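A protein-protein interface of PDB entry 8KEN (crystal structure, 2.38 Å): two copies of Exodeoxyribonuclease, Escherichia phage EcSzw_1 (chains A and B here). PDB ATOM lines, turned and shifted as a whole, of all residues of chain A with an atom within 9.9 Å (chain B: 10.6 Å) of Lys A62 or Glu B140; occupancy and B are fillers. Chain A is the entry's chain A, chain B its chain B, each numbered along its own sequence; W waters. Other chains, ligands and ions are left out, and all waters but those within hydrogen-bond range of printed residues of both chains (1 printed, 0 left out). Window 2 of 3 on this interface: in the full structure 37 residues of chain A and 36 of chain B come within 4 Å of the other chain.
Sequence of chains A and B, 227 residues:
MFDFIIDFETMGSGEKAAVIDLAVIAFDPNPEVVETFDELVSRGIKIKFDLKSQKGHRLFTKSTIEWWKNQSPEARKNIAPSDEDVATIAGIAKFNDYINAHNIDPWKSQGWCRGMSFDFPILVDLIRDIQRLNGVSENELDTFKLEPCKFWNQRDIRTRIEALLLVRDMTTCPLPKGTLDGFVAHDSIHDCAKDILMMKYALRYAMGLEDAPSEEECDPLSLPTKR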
ATOM      1  N   THR A  10     -17.145  16.563 -27.991  1.00  0.00           N
ATOM      2  CA  THR A  10     -18.456  16.365 -27.358  1.00  0.00           C
ATOM      3  C   THR A  10     -19.464  17.423 -27.798  1.00  0.00           C
ATOM      4  O   THR A  10     -19.127  18.433 -28.430  1.00  0.00           O
ATOM      5  CB  THR A  10     -18.406  16.415 -25.827  1.00  0.00           C
ATOM      6  OG1 THR A  10     -18.172  17.771 -25.397  1.00  0.00           O
ATOM      7  CG2 THR A  10     -17.333  15.493 -25.255  1.00  0.00           C
ATOM      8  N   MET A  11     -20.728  17.169 -27.444  1.00  0.00           N
ATOM      9  CA  MET A  11     -21.798  18.142 -27.608  1.00  0.00           C
ATOM     10  C   MET A  11     -22.292  18.706 -26.280  1.00  0.00           C
ATOM     11  O   MET A  11     -23.353  19.328 -26.241  1.00  0.00           O
ATOM     12  CB  MET A  11     -22.975  17.554 -28.367  1.00  0.00           C
ATOM     13  CG  MET A  11     -22.742  17.374 -29.816  1.00  0.00           C
ATOM     14  SD  MET A  11     -23.285  18.810 -30.713  1.00  0.00           S
ATOM     15  CE  MET A  11     -22.523  18.507 -32.312  1.00  0.00           C
ATOM     16  N   GLY A  12     -21.541  18.529 -25.205  1.00  0.00           N
ATOM     17  CA  GLY A  12     -21.961  19.018 -23.907  1.00  0.00           C
ATOM     18  C   GLY A  12     -20.807  18.893 -22.947  1.00  0.00           C
ATOM     19  O   GLY A  12     -19.701  18.513 -23.341  1.00  0.00           O
ATOM     20  N   SER A  13     -21.078  19.162 -21.658  1.00  0.00           N
ATOM     21  CA  SER A  13     -19.953  19.413 -20.761  1.00  0.00           C
ATOM     22  C   SER A  13     -19.788  18.427 -19.609  1.00  0.00           C
ATOM     23  O   SER A  13     -18.647  18.198 -19.189  1.00  0.00           O
ATOM     24  CB  SER A  13     -20.028  20.847 -20.185  1.00  0.00           C
ATOM     25  OG  SER A  13     -21.364  21.195 -19.814  1.00  0.00           O
ATOM     26  N   ALA A  18     -22.967  13.925 -24.557  1.00  0.00           N
ATOM     27  CA  ALA A  18     -22.942  13.307 -25.880  1.00  0.00           C
ATOM     28  C   ALA A  18     -21.561  13.472 -26.488  1.00  0.00           C
ATOM     29  O   ALA A  18     -21.010  14.572 -26.489  1.00  0.00           O
ATOM     30  CB  ALA A  18     -24.001  13.954 -26.785  1.00  0.00           C
ATOM     31  N   LYS A  55     -29.313  10.555 -28.630  1.00  0.00           N
ATOM     32  CA  LYS A  55     -30.459  11.404 -28.297  1.00  0.00           C
ATOM     33  C   LYS A  55     -31.364  10.643 -27.339  1.00  0.00           C
ATOM     34  O   LYS A  55     -31.699   9.479 -27.577  1.00  0.00           O
ATOM     35  CB  LYS A  55     -31.224  11.810 -29.563  1.00  0.00           C
ATOM     36  CG  LYS A  55     -30.607  12.986 -30.337  1.00  0.00           C
ATOM     37  CD  LYS A  55     -30.896  14.324 -29.629  1.00  0.00           C
ATOM     38  CE  LYS A  55     -30.068  15.473 -30.197  1.00  0.00           C
ATOM     39  NZ  LYS A  55     -30.017  15.448 -31.692  1.00  0.00           N
ATOM     40  N   LEU A  59     -26.151  13.978 -23.217  1.00  0.00           N
ATOM     41  CA  LEU A  59     -26.556  15.360 -22.953  1.00  0.00           C
ATOM     42  C   LEU A  59     -26.044  16.288 -24.051  1.00  0.00           C
ATOM     43  O   LEU A  59     -24.835  16.493 -24.184  1.00  0.00           O
ATOM     44  CB  LEU A  59     -26.037  15.794 -21.581  1.00  0.00           C
ATOM     45  CG  LEU A  59     -26.703  16.948 -20.829  1.00  0.00           C
ATOM     46  CD1 LEU A  59     -26.507  18.279 -21.528  1.00  0.00           C
ATOM     47  CD2 LEU A  59     -28.197  16.643 -20.630  1.00  0.00           C
ATOM     48  N   PHE A  60     -26.962  16.868 -24.825  1.00  0.00           N
ATOM     49  CA  PHE A  60     -26.613  17.850 -25.856  1.00  0.00           C
ATOM     50  C   PHE A  60     -26.831  19.246 -25.267  1.00  0.00           C
ATOM     51  O   PHE A  60     -27.952  19.748 -25.242  1.00  0.00           O
ATOM     52  CB  PHE A  60     -27.439  17.650 -27.129  1.00  0.00           C
ATOM     53  CG  PHE A  60     -27.172  16.342 -27.848  1.00  0.00           C
ATOM     54  CD1 PHE A  60     -27.749  15.155 -27.403  1.00  0.00           C
ATOM     55  CD2 PHE A  60     -26.356  16.306 -28.983  1.00  0.00           C
ATOM     56  CE1 PHE A  60     -27.513  13.957 -28.060  1.00  0.00           C
ATOM     57  CE2 PHE A  60     -26.108  15.111 -29.633  1.00  0.00           C
ATOM     58  CZ  PHE A  60     -26.698  13.930 -29.175  1.00  0.00           C
ATOM     59  N   THR A  61     -25.757  19.871 -24.796  1.00  0.00           N
ATOM     60  CA  THR A  61     -25.826  21.210 -24.236  1.00  0.00           C
ATOM     61  C   THR A  61     -25.946  22.235 -25.356  1.00  0.00           C
ATOM     62  O   THR A  61     -25.259  22.138 -26.377  1.00  0.00           O
ATOM     63  CB  THR A  61     -24.592  21.468 -23.375  1.00  0.00           C
ATOM     64  OG1 THR A  61     -24.664  20.642 -22.212  1.00  0.00           O
ATOM     65  CG2 THR A  61     -24.514  22.893 -22.935  1.00  0.00           C
ATOM     66  N   LYS A  62     -26.847  23.198 -25.181  1.00  0.00           N
ATOM     67  CA  LYS A  62     -27.125  24.136 -26.266  1.00  0.00           C
ATOM     68  C   LYS A  62     -26.012  25.167 -26.437  1.00  0.00           C
ATOM     69  O   LYS A  62     -25.736  25.597 -27.562  1.00  0.00           O
ATOM     70  CB  LYS A  62     -28.479  24.801 -26.026  1.00  0.00           C
ATOM     71  CG  LYS A  62     -29.611  23.768 -25.915  1.00  0.00           C
ATOM     72  CD  LYS A  62     -30.462  23.760 -27.168  1.00  0.00           C
ATOM     73  CE  LYS A  62     -31.616  24.773 -27.075  1.00  0.00           C
ATOM     74  NZ  LYS A  62     -32.626  24.395 -26.038  1.00  0.00           N
ATOM     75  N   SER A  63     -25.351  25.562 -25.354  1.00  0.00           N
ATOM     76  CA  SER A  63     -24.190  26.434 -25.487  1.00  0.00           C
ATOM     77  C   SER A  63     -23.009  25.742 -26.149  1.00  0.00           C
ATOM     78  O   SER A  63     -22.032  26.418 -26.494  1.00  0.00           O
ATOM     79  CB  SER A  63     -23.767  26.964 -24.121  1.00  0.00           C
ATOM     80  OG  SER A  63     -23.117  25.965 -23.362  1.00  0.00           O
ATOM     81  N   THR A  64     -23.058  24.417 -26.314  1.00  0.00           N
ATOM     82  CA  THR A  64     -22.051  23.685 -27.071  1.00  0.00           C
ATOM     83  C   THR A  64     -22.489  23.437 -28.503  1.00  0.00           C
ATOM     84  O   THR A  64     -21.663  23.503 -29.415  1.00  0.00           O
ATOM     85  CB  THR A  64     -21.736  22.357 -26.384  1.00  0.00           C
ATOM     86  OG1 THR A  64     -21.139  22.622 -25.109  1.00  0.00           O
ATOM     87  CG2 THR A  64     -20.742  21.528 -27.230  1.00  0.00           C
ATOM     88  N   ILE A  65     -23.782  23.182 -28.713  1.00  0.00           N
ATOM     89  CA  ILE A  65     -24.325  23.091 -30.066  1.00  0.00           C
ATOM     90  C   ILE A  65     -24.075  24.385 -30.824  1.00  0.00           C
ATOM     91  O   ILE A  65     -23.627  24.376 -31.980  1.00  0.00           O
ATOM     92  CB  ILE A  65     -25.823  22.757 -30.025  1.00  0.00           C
ATOM     93  CG1 ILE A  65     -26.045  21.329 -29.508  1.00  0.00           C
ATOM     94  CG2 ILE A  65     -26.427  22.959 -31.400  1.00  0.00           C
ATOM     95  CD1 ILE A  65     -27.461  21.079 -28.968  1.00  0.00           C
ATOM     96  N   GLU A  66     -24.352  25.525 -30.181  1.00  0.00           N
ATOM     97  CA  GLU A  66     -24.099  26.803 -30.832  1.00  0.00           C
ATOM     98  C   GLU A  66     -22.605  27.016 -31.055  1.00  0.00           C
ATOM     99  O   GLU A  66     -22.192  27.462 -32.131  1.00  0.00           O
ATOM    100  CB  GLU A  66     -24.712  27.941 -30.009  1.00  0.00           C
ATOM    101  N   TRP A  67     -21.776  26.685 -30.063  1.00  0.00           N
ATOM    102  CA  TRP A  67     -20.333  26.774 -30.259  1.00  0.00           C
ATOM    103  C   TRP A  67     -19.886  26.041 -31.528  1.00  0.00           C
ATOM    104  O   TRP A  67     -19.143  26.601 -32.341  1.00  0.00           O
ATOM    105  CB  TRP A  67     -19.601  26.227 -29.036  1.00  0.00           C
ATOM    106  CG  TRP A  67     -18.110  26.425 -29.121  1.00  0.00           C
ATOM    107  CD1 TRP A  67     -17.415  27.550 -28.767  1.00  0.00           C
ATOM    108  CD2 TRP A  67     -17.129  25.470 -29.560  1.00  0.00           C
ATOM    109  NE1 TRP A  67     -16.071  27.358 -28.966  1.00  0.00           N
ATOM    110  CE2 TRP A  67     -15.864  26.094 -29.453  1.00  0.00           C
ATOM    111  CE3 TRP A  67     -17.196  24.151 -30.035  1.00  0.00           C
ATOM    112  CZ2 TRP A  67     -14.672  25.451 -29.819  1.00  0.00           C
ATOM    113  CZ3 TRP A  67     -16.010  23.509 -30.389  1.00  0.00           C
ATOM    114  CH2 TRP A  67     -14.764  24.164 -30.278  1.00  0.00           C
ATOM    115  N   TRP A  68     -20.358  24.793 -31.732  1.00  0.00           N
ATOM    116  CA  TRP A  68     -19.980  24.045 -32.937  1.00  0.00           C
ATOM    117  C   TRP A  68     -20.487  24.735 -34.201  1.00  0.00           C
ATOM    118  O   TRP A  68     -19.777  24.787 -35.210  1.00  0.00           O
ATOM    119  CB  TRP A  68     -20.497  22.593 -32.880  1.00  0.00           C
ATOM    120  CG  TRP A  68     -19.610  21.645 -32.055  1.00  0.00           C
ATOM    121  CD1 TRP A  68     -19.950  21.009 -30.892  1.00  0.00           C
ATOM    122  CD2 TRP A  68     -18.259  21.240 -32.346  1.00  0.00           C
ATOM    123  NE1 TRP A  68     -18.889  20.259 -30.425  1.00  0.00           N
ATOM    124  CE2 TRP A  68     -17.842  20.380 -31.300  1.00  0.00           C
ATOM    125  CE3 TRP A  68     -17.356  21.535 -33.376  1.00  0.00           C
ATOM    126  CZ2 TRP A  68     -16.564  19.795 -31.266  1.00  0.00           C
ATOM    127  CZ3 TRP A  68     -16.088  20.953 -33.345  1.00  0.00           C
ATOM    128  CH2 TRP A  68     -15.704  20.096 -32.293  1.00  0.00           C
ATOM    129  N   LYS A  69     -21.711  25.276 -34.163  1.00  0.00           N
ATOM    130  CA  LYS A  69     -22.282  25.968 -35.316  1.00  0.00           C
ATOM    131  C   LYS A  69     -21.374  27.094 -35.822  1.00  0.00           C
ATOM    132  O   LYS A  69     -21.337  27.369 -37.028  1.00  0.00           O
ATOM    133  CB  LYS A  69     -23.643  26.548 -34.932  1.00  0.00           C
ATOM    134  CG  LYS A  69     -24.845  25.900 -35.587  1.00  0.00           C
ATOM    135  CD  LYS A  69     -26.125  26.338 -34.863  1.00  0.00           C
ATOM    136  CE  LYS A  69     -27.143  25.199 -34.753  1.00  0.00           C
ATOM    137  NZ  LYS A  69     -28.178  25.501 -33.705  1.00  0.00           N
ATOM    138  N   ASN A  70     -20.630  27.749 -34.928  1.00  0.00           N
ATOM    139  CA  ASN A  70     -19.796  28.881 -35.308  1.00  0.00           C
ATOM    140  C   ASN A  70     -18.379  28.498 -35.688  1.00  0.00           C
ATOM    141  O   ASN A  70     -17.596  29.385 -36.031  1.00  0.00           O
ATOM    142  CB  ASN A  70     -19.743  29.892 -34.165  1.00  0.00           C
ATOM    143  CG  ASN A  70     -21.079  30.531 -33.915  1.00  0.00           C
ATOM    144  OD1 ASN A  70     -21.756  30.945 -34.860  1.00  0.00           O
ATOM    145  ND2 ASN A  70     -21.491  30.586 -32.649  1.00  0.00           N
ATOM    146  N   ILE B 127     -22.680  23.379  -8.413  1.00  0.00           N
ATOM    147  CA  ILE B 127     -22.975  24.709  -8.931  1.00  0.00           C
ATOM    148  C   ILE B 127     -24.096  24.631  -9.966  1.00  0.00           C
ATOM    149  O   ILE B 127     -24.989  25.486  -9.988  1.00  0.00           O
ATOM    150  CB  ILE B 127     -21.693  25.358  -9.491  1.00  0.00           C
ATOM    151  CG1 ILE B 127     -20.726  25.705  -8.354  1.00  0.00           C
ATOM    152  CG2 ILE B 127     -22.024  26.571 -10.314  1.00  0.00           C
ATOM    153  CD1 ILE B 127     -19.308  25.938  -8.830  1.00  0.00           C
ATOM    154  N   ARG B 128     -24.090  23.590 -10.819  1.00  0.00           N
ATOM    155  CA  ARG B 128     -25.211  23.376 -11.741  1.00  0.00           C
ATOM    156  C   ARG B 128     -26.539  23.393 -11.002  1.00  0.00           C
ATOM    157  O   ARG B 128     -27.537  23.913 -11.509  1.00  0.00           O
ATOM    158  CB  ARG B 128     -25.072  22.036 -12.484  1.00  0.00           C
ATOM    159  CG  ARG B 128     -23.979  21.995 -13.542  1.00  0.00           C
ATOM    160  CD  ARG B 128     -24.255  20.949 -14.635  1.00  0.00           C
ATOM    161  NE  ARG B 128     -23.020  20.299 -15.055  1.00  0.00           N
ATOM    162  CZ  ARG B 128     -22.039  20.923 -15.698  1.00  0.00           C
ATOM    163  NH1 ARG B 128     -22.121  22.221 -16.000  1.00  0.00           N
ATOM    164  NH2 ARG B 128     -20.925  20.251 -15.988  1.00  0.00           N
ATOM    165  N   ILE B 130     -27.491  25.207  -8.698  1.00  0.00           N
ATOM    166  CA  ILE B 130     -27.971  26.592  -8.619  1.00  0.00           C
ATOM    167  C   ILE B 130     -28.833  26.917  -9.824  1.00  0.00           C
ATOM    168  O   ILE B 130     -29.897  27.536  -9.707  1.00  0.00           O
ATOM    169  CB  ILE B 130     -26.790  27.575  -8.521  1.00  0.00           C
ATOM    170  CG1 ILE B 130     -26.007  27.365  -7.237  1.00  0.00           C
ATOM    171  CG2 ILE B 130     -27.257  29.013  -8.692  1.00  0.00           C
ATOM    172  CD1 ILE B 130     -24.619  27.897  -7.320  1.00  0.00           C
ATOM    173  N   GLN B 131     -28.402  26.474 -11.003  1.00  0.00           N
ATOM    174  CA  GLN B 131     -29.150  26.786 -12.208  1.00  0.00           C
ATOM    175  C   GLN B 131     -30.406  25.938 -12.327  1.00  0.00           C
ATOM    176  O   GLN B 131     -31.423  26.420 -12.839  1.00  0.00           O
ATOM    177  CB  GLN B 131     -28.240  26.634 -13.429  1.00  0.00           C
ATOM    178  CG  GLN B 131     -27.684  27.972 -13.832  1.00  0.00           C
ATOM    179  CD  GLN B 131     -26.570  27.922 -14.833  1.00  0.00           C
ATOM    180  OE1 GLN B 131     -26.611  27.161 -15.795  1.00  0.00           O
ATOM    181  NE2 GLN B 131     -25.557  28.759 -14.624  1.00  0.00           N
ATOM    182  N   ARG B 132     -30.373  24.684 -11.860  1.00  0.00           N
ATOM    183  CA  ARG B 132     -31.602  23.895 -11.826  1.00  0.00           C
ATOM    184  C   ARG B 132     -32.581  24.466 -10.803  1.00  0.00           C
ATOM    185  O   ARG B 132     -33.797  24.462 -11.024  1.00  0.00           O
ATOM    186  CB  ARG B 132     -31.306  22.427 -11.507  1.00  0.00           C
ATOM    187  CG  ARG B 132     -30.229  21.753 -12.346  1.00  0.00           C
ATOM    188  CD  ARG B 132     -29.855  20.383 -11.742  1.00  0.00           C
ATOM    189  NE  ARG B 132     -28.849  19.708 -12.553  1.00  0.00           N
ATOM    190  CZ  ARG B 132     -27.620  19.398 -12.156  1.00  0.00           C
ATOM    191  NH1 ARG B 132     -27.193  19.674 -10.925  1.00  0.00           N
ATOM    192  NH2 ARG B 132     -26.788  18.811 -13.024  1.00  0.00           N
ATOM    193  N   ASN B 134     -33.097  27.481 -10.347  1.00  0.00           N
ATOM    194  CA  ASN B 134     -33.750  28.536 -11.127  1.00  0.00           C
ATOM    195  C   ASN B 134     -34.645  27.996 -12.241  1.00  0.00           C
ATOM    196  O   ASN B 134     -35.041  28.767 -13.119  1.00  0.00           O
ATOM    197  CB  ASN B 134     -32.703  29.466 -11.752  1.00  0.00           C
ATOM    198  CG  ASN B 134     -32.143  30.469 -10.763  1.00  0.00           C
ATOM    199  OD1 ASN B 134     -31.228  30.158  -9.989  1.00  0.00           O
ATOM    200  ND2 ASN B 134     -32.660  31.698 -10.806  1.00  0.00           N
ATOM    201  N   GLY B 135     -34.934  26.701 -12.266  1.00  0.00           N
ATOM    202  CA  GLY B 135     -35.732  26.141 -13.349  1.00  0.00           C
ATOM    203  C   GLY B 135     -35.050  25.971 -14.694  1.00  0.00           C
ATOM    204  O   GLY B 135     -35.738  25.806 -15.707  1.00  0.00           O
ATOM    205  N   VAL B 136     -33.733  26.003 -14.757  1.00  0.00           N
ATOM    206  CA  VAL B 136     -33.057  25.773 -16.031  1.00  0.00           C
ATOM    207  C   VAL B 136     -33.043  24.282 -16.366  1.00  0.00           C
ATOM    208  O   VAL B 136     -32.692  23.439 -15.528  1.00  0.00           O
ATOM    209  CB  VAL B 136     -31.640  26.358 -16.002  1.00  0.00           C
ATOM    210  CG1 VAL B 136     -30.878  25.978 -17.275  1.00  0.00           C
ATOM    211  CG2 VAL B 136     -31.747  27.876 -15.833  1.00  0.00           C
ATOM    212  N   SER B 137     -33.439  23.958 -17.601  1.00  0.00           N
ATOM    213  CA  SER B 137     -33.349  22.605 -18.143  1.00  0.00           C
ATOM    214  C   SER B 137     -31.911  22.090 -18.142  1.00  0.00           C
ATOM    215  O   SER B 137     -30.955  22.863 -18.255  1.00  0.00           O
ATOM    216  CB  SER B 137     -33.870  22.607 -19.576  1.00  0.00           C
ATOM    217  OG  SER B 137     -35.276  22.556 -19.595  1.00  0.00           O
ATOM    218  N   GLU B 138     -31.760  20.756 -18.072  1.00  0.00           N
ATOM    219  CA  GLU B 138     -30.425  20.159 -18.092  1.00  0.00           C
ATOM    220  C   GLU B 138     -29.675  20.509 -19.370  1.00  0.00           C
ATOM    221  O   GLU B 138     -28.453  20.700 -19.346  1.00  0.00           O
ATOM    222  CB  GLU B 138     -30.496  18.638 -17.954  1.00  0.00           C
ATOM    223  CG  GLU B 138     -30.720  18.102 -16.552  1.00  0.00           C
ATOM    224  CD  GLU B 138     -29.567  18.387 -15.600  1.00  0.00           C
ATOM    225  OE1 GLU B 138     -28.389  18.051 -15.884  1.00  0.00           O
ATOM    226  OE2 GLU B 138     -29.857  18.949 -14.535  1.00  0.00           O
ATOM    227  N   ASN B 139     -30.377  20.575 -20.496  1.00  0.00           N
ATOM    228  CA  ASN B 139     -29.678  20.780 -21.758  1.00  0.00           C
ATOM    229  C   ASN B 139     -29.357  22.235 -22.011  1.00  0.00           C
ATOM    230  O   ASN B 139     -28.812  22.550 -23.073  1.00  0.00           O
ATOM    231  CB  ASN B 139     -30.494  20.230 -22.941  1.00  0.00           C
ATOM    232  CG  ASN B 139     -31.722  21.054 -23.235  1.00  0.00           C
ATOM    233  OD1 ASN B 139     -32.203  21.773 -22.378  1.00  0.00           O
ATOM    234  ND2 ASN B 139     -32.247  20.939 -24.446  1.00  0.00           N
ATOM    235  N   GLU B 140     -29.690  23.122 -21.064  1.00  0.00           N
ATOM    236  CA  GLU B 140     -29.436  24.551 -21.194  1.00  0.00           C
ATOM    237  C   GLU B 140     -28.644  25.091 -20.017  1.00  0.00           C
ATOM    238  O   GLU B 140     -28.409  26.300 -19.950  1.00  0.00           O
ATOM    239  CB  GLU B 140     -30.748  25.345 -21.336  1.00  0.00           C
ATOM    240  CG  GLU B 140     -31.451  25.088 -22.663  1.00  0.00           C
ATOM    241  CD  GLU B 140     -32.610  26.030 -22.940  1.00  0.00           C
ATOM    242  OE1 GLU B 140     -33.349  25.761 -23.915  1.00  0.00           O
ATOM    243  OE2 GLU B 140     -32.775  27.033 -22.209  1.00  0.00           O
ATOM    244  N   LEU B 141     -28.231  24.228 -19.092  1.00  0.00           N
ATOM    245  CA  LEU B 141     -27.287  24.636 -18.063  1.00  0.00           C
ATOM    246  C   LEU B 141     -26.063  25.314 -18.682  1.00  0.00           C
ATOM    247  O   LEU B 141     -25.647  25.005 -19.808  1.00  0.00           O
ATOM    248  CB  LEU B 141     -26.866  23.420 -17.238  1.00  0.00           C
ATOM    249  CG  LEU B 141     -28.049  22.742 -16.560  1.00  0.00           C
ATOM    250  CD1 LEU B 141     -27.612  21.441 -15.914  1.00  0.00           C
ATOM    251  CD2 LEU B 141     -28.627  23.705 -15.520  1.00  0.00           C
ATOM    252  N   ASP B 142     -25.491  26.254 -17.929  1.00  0.00           N
ATOM    253  CA  ASP B 142     -24.306  27.003 -18.330  1.00  0.00           C
ATOM    254  C   ASP B 142     -23.749  27.729 -17.111  1.00  0.00           C
ATOM    255  O   ASP B 142     -24.200  28.837 -16.789  1.00  0.00           O
ATOM    256  CB  ASP B 142     -24.621  28.027 -19.432  1.00  0.00           C
ATOM    257  CG  ASP B 142     -23.354  28.661 -20.027  1.00  0.00           C
ATOM    258  OD1 ASP B 142     -22.612  29.369 -19.305  1.00  0.00           O
ATOM    259  OD2 ASP B 142     -23.081  28.403 -21.228  1.00  0.00           O
ATOM    260  N   THR B 143     -22.766  27.122 -16.443  1.00  0.00           N
ATOM    261  CA  THR B 143     -22.240  27.613 -15.177  1.00  0.00           C
ATOM    262  C   THR B 143     -20.935  28.371 -15.346  1.00  0.00           C
ATOM    263  O   THR B 143     -20.184  28.521 -14.374  1.00  0.00           O
ATOM    264  CB  THR B 143     -22.023  26.445 -14.216  1.00  0.00           C
ATOM    265  OG1 THR B 143     -21.102  25.519 -14.816  1.00  0.00           O
ATOM    266  CG2 THR B 143     -23.349  25.740 -13.894  1.00  0.00           C
ATOM    267  N   PHE B 144     -20.635  28.820 -16.563  1.00  0.00           N
ATOM    268  CA  PHE B 144     -19.313  29.363 -16.845  1.00  0.00           C
ATOM    269  C   PHE B 144     -19.021  30.596 -15.986  1.00  0.00           C
ATOM    270  O   PHE B 144     -17.902  30.761 -15.485  1.00  0.00           O
ATOM    271  CB  PHE B 144     -19.228  29.686 -18.329  1.00  0.00           C
ATOM    272  CG  PHE B 144     -17.925  30.280 -18.747  1.00  0.00           C
ATOM    273  CD1 PHE B 144     -16.765  29.530 -18.727  1.00  0.00           C
ATOM    274  CD2 PHE B 144     -17.854  31.614 -19.135  1.00  0.00           C
ATOM    275  CE1 PHE B 144     -15.550  30.076 -19.137  1.00  0.00           C
ATOM    276  CE2 PHE B 144     -16.644  32.181 -19.522  1.00  0.00           C
ATOM    277  CZ  PHE B 144     -15.488  31.400 -19.531  1.00  0.00           C
ATOM    278  N   LYS B 145     -20.014  31.462 -15.783  1.00  0.00           N
ATOM    279  CA  LYS B 145     -19.806  32.640 -14.952  1.00  0.00           C
ATOM    280  C   LYS B 145     -19.918  32.335 -13.466  1.00  0.00           C
ATOM    281  O   LYS B 145     -19.585  33.195 -12.650  1.00  0.00           O
ATOM    282  CB  LYS B 145     -20.808  33.750 -15.316  1.00  0.00           C
ATOM    283  CG  LYS B 145     -20.994  33.977 -16.822  1.00  0.00           C
ATOM    284  CD  LYS B 145     -22.041  32.995 -17.433  1.00  0.00           C
ATOM    285  CE  LYS B 145     -22.346  33.308 -18.905  1.00  0.00           C
ATOM    286  NZ  LYS B 145     -21.129  33.177 -19.778  1.00  0.00           N
ATOM    287  N   LEU B 146     -20.410  31.157 -13.088  1.00  0.00           N
ATOM    288  CA  LEU B 146     -20.543  30.829 -11.678  1.00  0.00           C
ATOM    289  C   LEU B 146     -19.369  30.038 -11.143  1.00  0.00           C
ATOM    290  O   LEU B 146     -19.272  29.860  -9.932  1.00  0.00           O
ATOM    291  CB  LEU B 146     -21.818  30.035 -11.418  1.00  0.00           C
ATOM    292  CG  LEU B 146     -23.148  30.718 -11.728  1.00  0.00           C
ATOM    293  CD1 LEU B 146     -24.231  29.668 -11.774  1.00  0.00           C
ATOM    294  CD2 LEU B 146     -23.451  31.785 -10.678  1.00  0.00           C
HETATM  295  O   HOH W   1     -26.029  25.574 -22.301  1.00  0.00           O
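Water W1 lies within hydrogen-bond range of the backbone carbonyl oxygen of Leu B141 (2.6 Å), the side-chain hydroxyl of Ser A63 (3.1 Å) and the backbone carbonyl oxygen of Glu B140 (3.4 Å).
Printed residues of chain B that touch a printed residue of chain A: Arg B128, Glu B138, Asn B139, Glu B140, Leu B141 and Asp B142.
Printed residues of chain A that touch a printed residue of chain B: Ser A13, Leu A59, Phe A60, Thr A61, Lys A62 and Ser A63.
Hydrophobic or aromatic side chains of chain A within 4 Å of the printed part of chain B: Leu A59.
Among the printed residues, 8 pairs touch across the chains.
Lys A62 touches just these residues of chain B: Asn B139 (3.0 Å) and Glu B140 (2.6 Å).
Of chain A, only Lys A62 (2.6 Å) comes within 4 Å of Glu B140.
Of chain B, only Asn B139 and Leu B141 come within 4 Å of Thr A61.
Of the printed residues of chain B, Ser A63 touches Asp B142 (3.2 Å).
No residue of chain B comes within 4 Å of Thr A64.
No residue of chain B comes within 4 Å of Ile A65.
No residue of chain B comes within 4 Å of Glu A66.
No residue of chain A comes within 4 Å of Ser B137.
Printed residues of chain A within 4 Å of Asp B142: Ser A63 (3.2 Å).
Printed residues of chain A within 4 Å of Arg B128: Ser A13.
Printed residues of chain B within 4 Å of Ser A13: Arg B128.
The nearest residue of chain A that does not touch Glu B140 is Thr A61 (5.4 Å).
The nearest printed residue of chain B that does not touch Ser A13 is Leu B141 (5.7 Å).
O of Asp B142 lies within hydrogen-bond range of NE2 of Gln B131 (2.6 Å).
OE1 of Glu B138 is in salt-bridge range of NH2 of Arg B132, at 3.4 Å.
The backbone NH of Phe B144 lies close to the side-chain carboxylate of Asp B142 (3.4 Å).
The backbone carbonyl oxygen of Met A11 is in hydrogen-bond range of the backbone NH of Thr A61.
The backbone carbonyl oxygen (O) of Leu A59 lies within hydrogen-bond range of the backbone NH (N) of Ala A18 (3.2 Å).
The backbone carbonyl oxygen (O) of Asn B139 is in hydrogen-bond range of the backbone NH (N) of Lys A62.
The side-chain carboxylate of Glu B140 lies within salt-bridge range of the side-chain amino group of Lys A62.
The side-chain hydroxyl of Ser A63 sits at hydrogen-bond distance from the side-chain carboxylate of Asp B142 (3.2 Å).
No position is printed for both chains.
Of the 8 pairs that touch across the chains among the printed residues, none has its exchanged pair printed and touching as well.
Ser A13 touches Arg B128.
Leu A59 touches Glu B138.
Asn B139 touches Phe A60.
Asn B139 touches Thr A61 (O to CA, 3.5 Å).
Leu B141 touches Thr A61.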
